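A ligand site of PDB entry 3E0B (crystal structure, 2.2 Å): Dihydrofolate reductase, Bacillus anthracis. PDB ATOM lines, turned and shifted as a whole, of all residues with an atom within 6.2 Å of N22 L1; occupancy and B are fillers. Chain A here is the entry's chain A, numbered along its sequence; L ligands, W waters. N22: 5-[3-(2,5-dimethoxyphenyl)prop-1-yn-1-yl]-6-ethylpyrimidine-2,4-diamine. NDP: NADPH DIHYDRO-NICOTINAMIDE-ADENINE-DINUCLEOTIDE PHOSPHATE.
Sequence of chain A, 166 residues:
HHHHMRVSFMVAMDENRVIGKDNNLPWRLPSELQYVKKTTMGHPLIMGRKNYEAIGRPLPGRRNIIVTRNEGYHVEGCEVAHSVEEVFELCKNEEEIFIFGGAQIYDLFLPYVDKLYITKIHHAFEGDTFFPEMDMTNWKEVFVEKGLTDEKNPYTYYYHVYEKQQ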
ATOM      1  N   MET A  10      -4.578 -30.807  12.940  1.00  0.00           N
ATOM      2  CA  MET A  10      -4.711 -29.583  13.704  1.00  0.00           C
ATOM      3  C   MET A  10      -4.055 -28.450  12.927  1.00  0.00           C
ATOM      4  O   MET A  10      -2.838 -28.419  12.752  1.00  0.00           O
ATOM      5  CB  MET A  10      -4.129 -29.746  15.107  1.00  0.00           C
ATOM      6  CG  MET A  10      -4.088 -28.465  15.957  1.00  0.00           C
ATOM      7  SD  MET A  10      -5.660 -27.648  16.358  1.00  0.00           S
ATOM      8  CE  MET A  10      -6.426 -28.814  17.499  1.00  0.00           C
ATOM      9  N   VAL A  11      -4.888 -27.499  12.480  1.00  0.00           N
ATOM     10  CA  VAL A  11      -4.398 -26.423  11.612  1.00  0.00           C
ATOM     11  C   VAL A  11      -5.193 -25.121  11.722  1.00  0.00           C
ATOM     12  O   VAL A  11      -6.378 -25.109  12.075  1.00  0.00           O
ATOM     13  CB  VAL A  11      -4.330 -26.905  10.108  1.00  0.00           C
ATOM     14  CG1 VAL A  11      -5.723 -27.116   9.545  1.00  0.00           C
ATOM     15  CG2 VAL A  11      -3.546 -25.926   9.239  1.00  0.00           C
ATOM     16  N   ALA A  12      -4.506 -24.009  11.454  1.00  0.00           N
ATOM     17  CA  ALA A  12      -5.126 -22.686  11.390  1.00  0.00           C
ATOM     18  C   ALA A  12      -4.728 -22.064  10.043  1.00  0.00           C
ATOM     19  O   ALA A  12      -3.534 -22.023   9.690  1.00  0.00           O
ATOM     20  CB  ALA A  12      -4.634 -21.832  12.537  1.00  0.00           C
ATOM     21  N   ASN A  23       8.821 -19.254   6.585  1.00  0.00           N
ATOM     22  CA  ASN A  23       9.090 -20.310   7.566  1.00  0.00           C
ATOM     23  C   ASN A  23       8.620 -19.957   9.002  1.00  0.00           C
ATOM     24  O   ASN A  23       9.202 -20.385   9.983  1.00  0.00           O
ATOM     25  CB  ASN A  23      10.574 -20.694   7.531  1.00  0.00           C
ATOM     26  CG  ASN A  23      10.823 -22.081   8.048  1.00  0.00           C
ATOM     27  OD1 ASN A  23      10.015 -22.991   7.867  1.00  0.00           O
ATOM     28  ND2 ASN A  23      11.974 -22.262   8.696  1.00  0.00           N
ATOM     29  N   ASN A  24       7.519 -19.199   9.092  1.00  0.00           N
ATOM     30  CA  ASN A  24       6.911 -18.832  10.371  1.00  0.00           C
ATOM     31  C   ASN A  24       5.400 -18.630  10.182  1.00  0.00           C
ATOM     32  O   ASN A  24       4.861 -18.829   9.075  1.00  0.00           O
ATOM     33  CB  ASN A  24       7.551 -17.532  10.878  1.00  0.00           C
ATOM     34  CG  ASN A  24       7.503 -17.378  12.424  1.00  0.00           C
ATOM     35  OD1 ASN A  24       6.539 -17.778  13.078  1.00  0.00           O
ATOM     36  ND2 ASN A  24       8.532 -16.736  12.981  1.00  0.00           N
ATOM     37  N   LEU A  25       4.732 -18.268  11.257  1.00  0.00           N
ATOM     38  CA  LEU A  25       3.283 -17.958  11.265  1.00  0.00           C
ATOM     39  C   LEU A  25       3.045 -16.505  10.794  1.00  0.00           C
ATOM     40  O   LEU A  25       3.777 -15.606  11.201  1.00  0.00           O
ATOM     41  CB  LEU A  25       2.768 -18.099  12.697  1.00  0.00           C
ATOM     42  CG  LEU A  25       2.067 -19.393  13.141  1.00  0.00           C
ATOM     43  CD1 LEU A  25       2.195 -20.579  12.153  1.00  0.00           C
ATOM     44  CD2 LEU A  25       2.460 -19.757  14.580  1.00  0.00           C
ATOM     45  N   TRP A  27       0.512 -14.653  11.591  1.00  0.00           N
ATOM     46  CA  TRP A  27      -0.320 -13.935  12.559  1.00  0.00           C
ATOM     47  C   TRP A  27       0.057 -14.348  13.965  1.00  0.00           C
ATOM     48  O   TRP A  27       0.694 -15.379  14.167  1.00  0.00           O
ATOM     49  CB  TRP A  27      -1.807 -14.286  12.338  1.00  0.00           C
ATOM     50  CG  TRP A  27      -2.047 -15.790  12.321  1.00  0.00           C
ATOM     51  CD1 TRP A  27      -2.121 -16.621  13.410  1.00  0.00           C
ATOM     52  CD2 TRP A  27      -2.199 -16.622  11.163  1.00  0.00           C
ATOM     53  NE1 TRP A  27      -2.322 -17.926  13.000  1.00  0.00           N
ATOM     54  CE2 TRP A  27      -2.392 -17.943  11.623  1.00  0.00           C
ATOM     55  CE3 TRP A  27      -2.195 -16.380   9.778  1.00  0.00           C
ATOM     56  CZ2 TRP A  27      -2.578 -19.031  10.741  1.00  0.00           C
ATOM     57  CZ3 TRP A  27      -2.388 -17.460   8.905  1.00  0.00           C
ATOM     58  CH2 TRP A  27      -2.553 -18.767   9.394  1.00  0.00           C
ATOM     59  N   GLU A  32      -5.966 -18.502  20.324  1.00  0.00           N
ATOM     60  CA  GLU A  32      -6.075 -19.627  19.412  1.00  0.00           C
ATOM     61  C   GLU A  32      -5.060 -20.707  19.761  1.00  0.00           C
ATOM     62  O   GLU A  32      -5.341 -21.908  19.622  1.00  0.00           O
ATOM     63  CB  GLU A  32      -5.894 -19.130  17.977  1.00  0.00           C
ATOM     64  CG  GLU A  32      -6.490 -20.021  16.886  1.00  0.00           C
ATOM     65  CD  GLU A  32      -5.645 -21.251  16.551  1.00  0.00           C
ATOM     66  OE1 GLU A  32      -4.404 -21.159  16.622  1.00  0.00           O
ATOM     67  OE2 GLU A  32      -6.217 -22.304  16.204  1.00  0.00           O
ATOM     68  N   LEU A  33      -3.868 -20.271  20.201  1.00  0.00           N
ATOM     69  CA  LEU A  33      -2.817 -21.188  20.666  1.00  0.00           C
ATOM     70  C   LEU A  33      -3.240 -21.907  21.943  1.00  0.00           C
ATOM     71  O   LEU A  33      -2.831 -23.051  22.179  1.00  0.00           O
ATOM     72  CB  LEU A  33      -1.520 -20.419  20.898  1.00  0.00           C
ATOM     73  CG  LEU A  33      -0.292 -21.278  21.157  1.00  0.00           C
ATOM     74  CD1 LEU A  33       0.099 -22.070  19.901  1.00  0.00           C
ATOM     75  CD2 LEU A  33       0.905 -20.442  21.701  1.00  0.00           C
ATOM     76  N   TYR A  35      -6.350 -22.727  22.610  1.00  0.00           N
ATOM     77  CA  TYR A  35      -7.308 -23.727  22.163  1.00  0.00           C
ATOM     78  C   TYR A  35      -6.569 -24.941  21.626  1.00  0.00           C
ATOM     79  O   TYR A  35      -6.957 -26.083  21.865  1.00  0.00           O
ATOM     80  CB  TYR A  35      -8.248 -23.137  21.118  1.00  0.00           C
ATOM     81  CG  TYR A  35      -9.060 -24.162  20.342  1.00  0.00           C
ATOM     82  CD1 TYR A  35      -8.541 -24.705  19.170  1.00  0.00           C
ATOM     83  CD2 TYR A  35     -10.331 -24.570  20.745  1.00  0.00           C
ATOM     84  CE1 TYR A  35      -9.230 -25.619  18.437  1.00  0.00           C
ATOM     85  CE2 TYR A  35     -11.047 -25.508  20.003  1.00  0.00           C
ATOM     86  CZ  TYR A  35     -10.472 -25.999  18.814  1.00  0.00           C
ATOM     87  OH  TYR A  35     -11.110 -26.882  17.990  1.00  0.00           O
ATOM     88  N   VAL A  36      -5.465 -24.682  20.919  1.00  0.00           N
ATOM     89  CA  VAL A  36      -4.615 -25.740  20.408  1.00  0.00           C
ATOM     90  C   VAL A  36      -4.018 -26.588  21.536  1.00  0.00           C
ATOM     91  O   VAL A  36      -3.996 -27.816  21.457  1.00  0.00           O
ATOM     92  CB  VAL A  36      -3.485 -25.164  19.519  1.00  0.00           C
ATOM     93  CG1 VAL A  36      -2.424 -26.214  19.252  1.00  0.00           C
ATOM     94  CG2 VAL A  36      -4.061 -24.624  18.220  1.00  0.00           C
ATOM     95  N   LEU A  45       1.962 -35.221  18.994  1.00  0.00           N
ATOM     96  CA  LEU A  45       2.037 -34.151  17.969  1.00  0.00           C
ATOM     97  C   LEU A  45       3.006 -34.618  16.882  1.00  0.00           C
ATOM     98  O   LEU A  45       4.151 -34.963  17.185  1.00  0.00           O
ATOM     99  CB  LEU A  45       2.590 -32.871  18.583  1.00  0.00           C
ATOM    100  CG  LEU A  45       1.688 -31.665  18.779  1.00  0.00           C
ATOM    101  CD1 LEU A  45       0.213 -32.021  18.997  1.00  0.00           C
ATOM    102  CD2 LEU A  45       2.228 -30.722  19.858  1.00  0.00           C
ATOM    103  N   ASN A  51       8.534 -27.319  10.448  1.00  0.00           N
ATOM    104  CA  ASN A  51       7.633 -26.867  11.511  1.00  0.00           C
ATOM    105  C   ASN A  51       8.328 -27.002  12.874  1.00  0.00           C
ATOM    106  O   ASN A  51       8.402 -26.043  13.629  1.00  0.00           O
ATOM    107  CB  ASN A  51       6.312 -27.640  11.515  1.00  0.00           C
ATOM    108  CG  ASN A  51       5.373 -27.163  12.615  1.00  0.00           C
ATOM    109  OD1 ASN A  51       5.456 -26.010  13.046  1.00  0.00           O
ATOM    110  ND2 ASN A  51       4.521 -28.057  13.116  1.00  0.00           N
ATOM    111  N   ALA A  54      10.981 -24.316  13.648  1.00  0.00           N
ATOM    112  CA  ALA A  54      10.407 -23.000  13.842  1.00  0.00           C
ATOM    113  C   ALA A  54       9.861 -22.870  15.284  1.00  0.00           C
ATOM    114  O   ALA A  54      10.068 -21.858  15.936  1.00  0.00           O
ATOM    115  CB  ALA A  54       9.327 -22.710  12.807  1.00  0.00           C
ATOM    116  N   ILE A  55       9.220 -23.926  15.795  1.00  0.00           N
ATOM    117  CA  ILE A  55       8.764 -23.978  17.177  1.00  0.00           C
ATOM    118  C   ILE A  55       9.995 -23.914  18.107  1.00  0.00           C
ATOM    119  O   ILE A  55      10.027 -23.116  19.055  1.00  0.00           O
ATOM    120  CB  ILE A  55       7.951 -25.279  17.449  1.00  0.00           C
ATOM    121  CG1 ILE A  55       6.717 -25.317  16.537  1.00  0.00           C
ATOM    122  CG2 ILE A  55       7.588 -25.385  18.926  1.00  0.00           C
ATOM    123  CD1 ILE A  55       5.926 -26.600  16.568  1.00  0.00           C
ATOM    124  N   LEU A  59       7.118 -29.551  22.883  1.00  0.00           N
ATOM    125  CA  LEU A  59       5.923 -29.019  23.528  1.00  0.00           C
ATOM    126  C   LEU A  59       5.533 -29.957  24.680  1.00  0.00           C
ATOM    127  O   LEU A  59       5.309 -31.154  24.481  1.00  0.00           O
ATOM    128  CB  LEU A  59       4.791 -28.862  22.511  1.00  0.00           C
ATOM    129  CG  LEU A  59       5.099 -27.860  21.382  1.00  0.00           C
ATOM    130  CD1 LEU A  59       4.103 -27.941  20.258  1.00  0.00           C
ATOM    131  CD2 LEU A  59       5.196 -26.428  21.905  1.00  0.00           C
ATOM    132  N   ARG A  62       3.137 -33.859  25.787  1.00  0.00           N
ATOM    133  CA  ARG A  62       2.769 -34.512  24.514  1.00  0.00           C
ATOM    134  C   ARG A  62       3.998 -35.223  23.951  1.00  0.00           C
ATOM    135  O   ARG A  62       5.109 -34.760  24.153  1.00  0.00           O
ATOM    136  CB  ARG A  62       2.292 -33.448  23.494  1.00  0.00           C
ATOM    137  CG  ARG A  62       0.818 -33.070  23.585  1.00  0.00           C
ATOM    138  CD  ARG A  62       0.564 -31.624  23.185  1.00  0.00           C
ATOM    139  NE  ARG A  62       1.388 -30.698  23.973  1.00  0.00           N
ATOM    140  CZ  ARG A  62       1.237 -29.374  23.978  1.00  0.00           C
ATOM    141  NH1 ARG A  62       0.300 -28.802  23.236  1.00  0.00           N
ATOM    142  NH2 ARG A  62       2.040 -28.598  24.715  1.00  0.00           N
ATOM    143  N   ILE A  99      -1.786 -34.408  13.598  1.00  0.00           N
ATOM    144  CA  ILE A  99      -0.902 -33.952  12.551  1.00  0.00           C
ATOM    145  C   ILE A  99      -0.910 -32.438  12.661  1.00  0.00           C
ATOM    146  O   ILE A  99      -1.919 -31.772  12.402  1.00  0.00           O
ATOM    147  CB  ILE A  99      -1.386 -34.447  11.114  1.00  0.00           C
ATOM    148  CG1 ILE A  99      -1.703 -35.955  11.142  1.00  0.00           C
ATOM    149  CG2 ILE A  99      -0.352 -34.070  10.020  1.00  0.00           C
ATOM    150  CD1 ILE A  99      -0.532 -36.862  11.578  1.00  0.00           C
ATOM    151  N   PHE A 100       0.261 -31.905  12.974  1.00  0.00           N
ATOM    152  CA  PHE A 100       0.400 -30.548  13.400  1.00  0.00           C
ATOM    153  C   PHE A 100       1.106 -29.656  12.368  1.00  0.00           C
ATOM    154  O   PHE A 100       1.483 -28.506  12.669  1.00  0.00           O
ATOM    155  CB  PHE A 100       1.183 -30.606  14.703  1.00  0.00           C
ATOM    156  CG  PHE A 100       1.021 -29.423  15.592  1.00  0.00           C
ATOM    157  CD1 PHE A 100      -0.213 -29.114  16.127  1.00  0.00           C
ATOM    158  CD2 PHE A 100       2.152 -28.734  16.049  1.00  0.00           C
ATOM    159  CE1 PHE A 100      -0.352 -28.042  17.027  1.00  0.00           C
ATOM    160  CE2 PHE A 100       2.029 -27.671  16.935  1.00  0.00           C
ATOM    161  CZ  PHE A 100       0.760 -27.325  17.434  1.00  0.00           C
ATOM    162  N   GLY A 101       1.304 -30.173  11.145  1.00  0.00           N
ATOM    163  CA  GLY A 101       1.937 -29.408  10.056  1.00  0.00           C
ATOM    164  C   GLY A 101       3.455 -29.528   9.947  1.00  0.00           C
ATOM    165  O   GLY A 101       4.088 -30.221  10.751  1.00  0.00           O
ATOM    166  N   TYR A 106       1.206 -32.168   6.145  1.00  0.00           N
ATOM    167  CA  TYR A 106      -0.239 -32.290   5.919  1.00  0.00           C
ATOM    168  C   TYR A 106      -0.521 -33.092   4.661  1.00  0.00           C
ATOM    169  O   TYR A 106      -1.444 -33.899   4.650  1.00  0.00           O
ATOM    170  CB  TYR A 106      -0.930 -30.914   5.798  1.00  0.00           C
ATOM    171  CG  TYR A 106      -1.045 -30.150   7.105  1.00  0.00           C
ATOM    172  CD1 TYR A 106      -1.535 -30.751   8.258  1.00  0.00           C
ATOM    173  CD2 TYR A 106      -0.745 -28.797   7.153  1.00  0.00           C
ATOM    174  CE1 TYR A 106      -1.646 -30.059   9.427  1.00  0.00           C
ATOM    175  CE2 TYR A 106      -0.846 -28.096   8.321  1.00  0.00           C
ATOM    176  CZ  TYR A 106      -1.311 -28.727   9.454  1.00  0.00           C
ATOM    177  OH  TYR A 106      -1.418 -28.016  10.632  1.00  0.00           O
ATOM    178  N   TYR A 117      -9.489 -30.511  12.825  1.00  0.00           N
ATOM    179  CA  TYR A 117      -9.664 -29.336  13.691  1.00  0.00           C
ATOM    180  C   TYR A 117      -9.000 -28.188  12.971  1.00  0.00           C
ATOM    181  O   TYR A 117      -7.760 -28.061  12.944  1.00  0.00           O
ATOM    182  CB  TYR A 117      -8.994 -29.508  15.048  1.00  0.00           C
ATOM    183  CG  TYR A 117      -9.463 -30.698  15.861  1.00  0.00           C
ATOM    184  CD1 TYR A 117      -9.129 -31.995  15.496  1.00  0.00           C
ATOM    185  CD2 TYR A 117     -10.189 -30.507  17.041  1.00  0.00           C
ATOM    186  CE1 TYR A 117      -9.552 -33.091  16.258  1.00  0.00           C
ATOM    187  CE2 TYR A 117     -10.608 -31.586  17.811  1.00  0.00           C
ATOM    188  CZ  TYR A 117     -10.266 -32.873  17.421  1.00  0.00           C
ATOM    189  OH  TYR A 117     -10.686 -33.942  18.171  1.00  0.00           O
ATOM    190  N   ILE A 118      -9.829 -27.339  12.381  1.00  0.00           N
ATOM    191  CA  ILE A 118      -9.355 -26.261  11.564  1.00  0.00           C
ATOM    192  C   ILE A 118      -9.898 -24.903  12.015  1.00  0.00           C
ATOM    193  O   ILE A 118     -11.117 -24.710  12.167  1.00  0.00           O
ATOM    194  CB  ILE A 118      -9.610 -26.539  10.064  1.00  0.00           C
ATOM    195  CG1 ILE A 118      -8.989 -25.463   9.182  1.00  0.00           C
ATOM    196  CG2 ILE A 118     -11.108 -26.695   9.743  1.00  0.00           C
ATOM    197  CD1 ILE A 118      -8.910 -25.879   7.724  1.00  0.00           C
ATOM    198  N   THR A 119      -8.965 -24.005  12.310  1.00  0.00           N
ATOM    199  CA  THR A 119      -9.305 -22.644  12.611  1.00  0.00           C
ATOM    200  C   THR A 119      -9.253 -21.839  11.322  1.00  0.00           C
ATOM    201  O   THR A 119      -8.271 -21.905  10.575  1.00  0.00           O
ATOM    202  CB  THR A 119      -8.368 -22.026  13.646  1.00  0.00           C
ATOM    203  OG1 THR A 119      -8.299 -22.893  14.796  1.00  0.00           O
ATOM    204  CG2 THR A 119      -8.864 -20.625  14.080  1.00  0.00           C
HETATM  205  C8  N22 L   1      -1.024 -20.943  14.689  1.00  0.00           C
HETATM  206  C7  N22 L   1      -1.032 -21.964  15.794  1.00  0.00           C
HETATM  207  C5  N22 L   1      -1.676 -23.260  15.280  1.00  0.00           C
HETATM  208  N4  N22 L   1      -3.008 -23.355  15.330  1.00  0.00           N
HETATM  209  C3  N22 L   1      -3.659 -24.472  14.940  1.00  0.00           C
HETATM  210  N8  N22 L   1      -5.005 -24.496  15.014  1.00  0.00           N
HETATM  211  N2  N22 L   1      -2.969 -25.529  14.475  1.00  0.00           N
HETATM  212  C1  N22 L   1      -1.633 -25.495  14.386  1.00  0.00           C
HETATM  213  N7  N22 L   1      -0.958 -26.563  13.951  1.00  0.00           N
HETATM  214  C6  N22 L   1      -0.941 -24.347  14.809  1.00  0.00           C
HETATM  215  C9  N22 L   1       0.505 -24.252  14.755  1.00  0.00           C
HETATM  216  C10 N22 L   1       1.753 -24.078  14.767  1.00  0.00           C
HETATM  217  C11 N22 L   1       3.210 -23.801  14.750  1.00  0.00           C
HETATM  218  C13 N22 L   1       3.729 -23.248  16.094  1.00  0.00           C
HETATM  219  C18 N22 L   1       3.222 -23.771  17.304  1.00  0.00           C
HETATM  220  C17 N22 L   1       3.688 -23.306  18.549  1.00  0.00           C
HETATM  221  O2  N22 L   1       3.213 -23.801  19.756  1.00  0.00           O
HETATM  222  C4  N22 L   1       2.231 -24.831  19.623  1.00  0.00           C
HETATM  223  C16 N22 L   1       4.673 -22.332  18.582  1.00  0.00           C
HETATM  224  C15 N22 L   1       5.189 -21.817  17.387  1.00  0.00           C
HETATM  225  C14 N22 L   1       4.738 -22.277  16.149  1.00  0.00           C
HETATM  226  O10 N22 L   1       5.262 -21.781  14.966  1.00  0.00           O
HETATM  227  C2  N22 L   1       6.401 -20.929  15.094  1.00  0.00           C
HETATM  228  PA  NDP L   2       7.054 -29.081   7.057  1.00  0.00           P
HETATM  229  O1A NDP L   2       5.998 -29.844   6.364  1.00  0.00           O
HETATM  230  O2A NDP L   2       6.797 -28.859   8.508  1.00  0.00           O
HETATM  231  O5B NDP L   2       8.425 -29.875   6.990  1.00  0.00           O
HETATM  232  C5B NDP L   2       8.938 -30.278   5.761  1.00  0.00           C
HETATM  233  C4B NDP L   2      10.002 -31.273   6.145  1.00  0.00           C
HETATM  234  O4B NDP L   2       9.365 -32.485   6.507  1.00  0.00           O
HETATM  235  C3B NDP L   2      10.954 -31.627   5.018  1.00  0.00           C
HETATM  236  O3B NDP L   2      12.002 -30.713   4.936  1.00  0.00           O
HETATM  237  C2B NDP L   2      11.413 -33.003   5.439  1.00  0.00           C
HETATM  238  O2B NDP L   2      12.440 -32.886   6.421  1.00  0.00           O
HETATM  239  C1B NDP L   2      10.167 -33.563   6.132  1.00  0.00           C
HETATM  240  N9A NDP L   2       9.440 -34.350   5.144  1.00  0.00           N
HETATM  241  C8A NDP L   2       8.614 -33.895   4.144  1.00  0.00           C
HETATM  242  N7A NDP L   2       8.129 -34.970   3.467  1.00  0.00           N
HETATM  243  C5A NDP L   2       8.655 -36.088   4.028  1.00  0.00           C
HETATM  244  C6A NDP L   2       8.540 -37.439   3.722  1.00  0.00           C
HETATM  245  N6A NDP L   2       7.779 -37.837   2.712  1.00  0.00           N
HETATM  246  N1A NDP L   2       9.218 -38.367   4.502  1.00  0.00           N
HETATM  247  C2A NDP L   2      10.007 -37.974   5.559  1.00  0.00           C
HETATM  248  N3A NDP L   2      10.122 -36.636   5.843  1.00  0.00           N
HETATM  249  C4A NDP L   2       9.478 -35.712   5.080  1.00  0.00           C
HETATM  250  O3  NDP L   2       7.459 -27.758   6.205  1.00  0.00           O
HETATM  251  PN  NDP L   2       6.640 -26.683   5.297  1.00  0.00           P
HETATM  252  O1N NDP L   2       7.586 -25.699   4.726  1.00  0.00           O
HETATM  253  O2N NDP L   2       5.805 -27.440   4.366  1.00  0.00           O
HETATM  254  O5D NDP L   2       5.675 -25.962   6.415  1.00  0.00           O
HETATM  255  C5D NDP L   2       6.229 -25.137   7.426  1.00  0.00           C
HETATM  256  C4D NDP L   2       5.493 -23.800   7.481  1.00  0.00           C
HETATM  257  O4D NDP L   2       4.145 -23.951   7.876  1.00  0.00           O
HETATM  258  C3D NDP L   2       6.098 -22.821   8.476  1.00  0.00           C
HETATM  259  O3D NDP L   2       5.876 -21.531   7.937  1.00  0.00           O
HETATM  260  C2D NDP L   2       5.210 -22.946   9.684  1.00  0.00           C
HETATM  261  O2D NDP L   2       5.318 -21.799  10.478  1.00  0.00           O
HETATM  262  C1D NDP L   2       3.845 -23.135   9.012  1.00  0.00           C
HETATM  263  N1N NDP L   2       2.866 -23.865   9.848  1.00  0.00           N
HETATM  264  C2N NDP L   2       1.619 -23.316  10.046  1.00  0.00           C
HETATM  265  C3N NDP L   2       0.666 -24.019  10.789  1.00  0.00           C
HETATM  266  C7N NDP L   2      -0.682 -23.427  11.037  1.00  0.00           C
HETATM  267  O7N NDP L   2      -1.661 -24.234  11.628  1.00  0.00           O
HETATM  268  N7N NDP L   2      -0.940 -22.166  10.673  1.00  0.00           N
HETATM  269  C4N NDP L   2       0.982 -25.279  11.315  1.00  0.00           C
HETATM  270  C5N NDP L   2       2.238 -25.827  11.112  1.00  0.00           C
HETATM  271  C6N NDP L   2       3.175 -25.106  10.362  1.00  0.00           C
HETATM  272  P2B NDP L   2      14.005 -32.952   6.079  1.00  0.00           P
HETATM  273  O1X NDP L   2      14.296 -34.247   5.321  1.00  0.00           O
HETATM  274  O2X NDP L   2      14.297 -31.759   5.219  1.00  0.00           O
HETATM  275  O3X NDP L   2      14.781 -32.835   7.346  1.00  0.00           O
HETATM  276  O   HOH W   1      -3.015 -19.025  15.310  1.00  0.00           O
HETATM  277  O   HOH W   2      -8.061 -25.717  14.879  1.00  0.00           O
HETATM  278  O   HOH W   3       6.004 -23.307  12.592  1.00  0.00           O
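A nitrogen (N7) of N22 L1 lies close to an oxygen (O7N) of NDP L2 (3.4 Å).
Water W1 bridges the indole nitrogen of Trp 27 (2.7 Å) and the side-chain carboxylate of Glu 32 (2.9 Å). Water W3 lies within hydrogen-bond range of O2D of NDP L2 (2.7 Å), OD1 of Asn 51 (2.8 Å) and O10 of N22 L1 (2.9 Å).
A nitrogen (N8) of N22 L1 lies within hydrogen-bond range of the side-chain carboxylate of Glu 32, 2.8 Å away. O of Met 10 lies within hydrogen-bond range of N7 of N22 L1 (2.9 Å). The side-chain sulfur of Met 10 sits at hydrogen-bond distance from a nitrogen (N8) of N22 L1, at 3.5 Å. N of Val 11 sits close to N2 of N22 L1. The backbone carbonyl oxygen (O) of Val 11 lies within hydrogen-bond range of a nitrogen (N8) of N22 L1 (3.3 Å). O of Phe 100 sits at hydrogen-bond distance from N7 of N22 L1 (3.4 Å). The backbone NH (N) of Ala 12 sits at hydrogen-bond distance from an oxygen (O7N) of NDP L2 (2.9 Å). The backbone carbonyl oxygen (O) of Ala 12 is in hydrogen-bond range of a nitrogen (N7N) of NDP L2, 2.8 Å away. The backbone NH (N) of Asn 51 lies within hydrogen-bond range of an oxygen (O2A) of NDP L2 (3.0 Å). N of Asn 24 is in hydrogen-bond range of O3D of NDP L2, 3.1 Å away. O of Asn 24 is in hydrogen-bond range of O3D of NDP L2 (3.1 Å).
OE2 of Glu 32 lies within hydrogen-bond range of OG1 of Thr 119 (2.6 Å). The backbone carbonyl oxygen of Met 10 is in hydrogen-bond range of the side-chain hydroxyl of Tyr 106, at 2.6 Å. O of Ile 99 sits at hydrogen-bond distance from N of Met 10 (2.9 Å). The backbone carbonyl oxygen of Val 11 is in hydrogen-bond range of the backbone NH of Thr 119 (2.8 Å). The backbone carbonyl oxygen (O) of Tyr 117 sits at hydrogen-bond distance from the backbone NH (N) of Val 11. ND2 of Asn 51 lies within hydrogen-bond range of O of Phe 100, at 3.1 Å. The side-chain amide nitrogen of Asn 51 is in hydrogen-bond range of the backbone carbonyl oxygen of Gly 101, 3.2 Å away.
Merely in contact with N22 L1: Ala 12 (3.6 Å), Asn 24 (3.7 Å), Leu 25 (3.5 Å), Trp 27 (3.7 Å), Leu 33 (3.5 Å), Val 36 (3.3 Å), Asn 51 (3.6 Å), Ala 54 (3.9 Å), Ile 55 (3.6 Å), Leu 59 (3.7 Å), Tyr 106 (3.7 Å) and Thr 119 (3.7 Å). Of the 24 residues printed, 16 come within 4 Å of N22 L1. The nearest printed residue that does not touch N22 L1 is Tyr 117 (5.0 Å).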
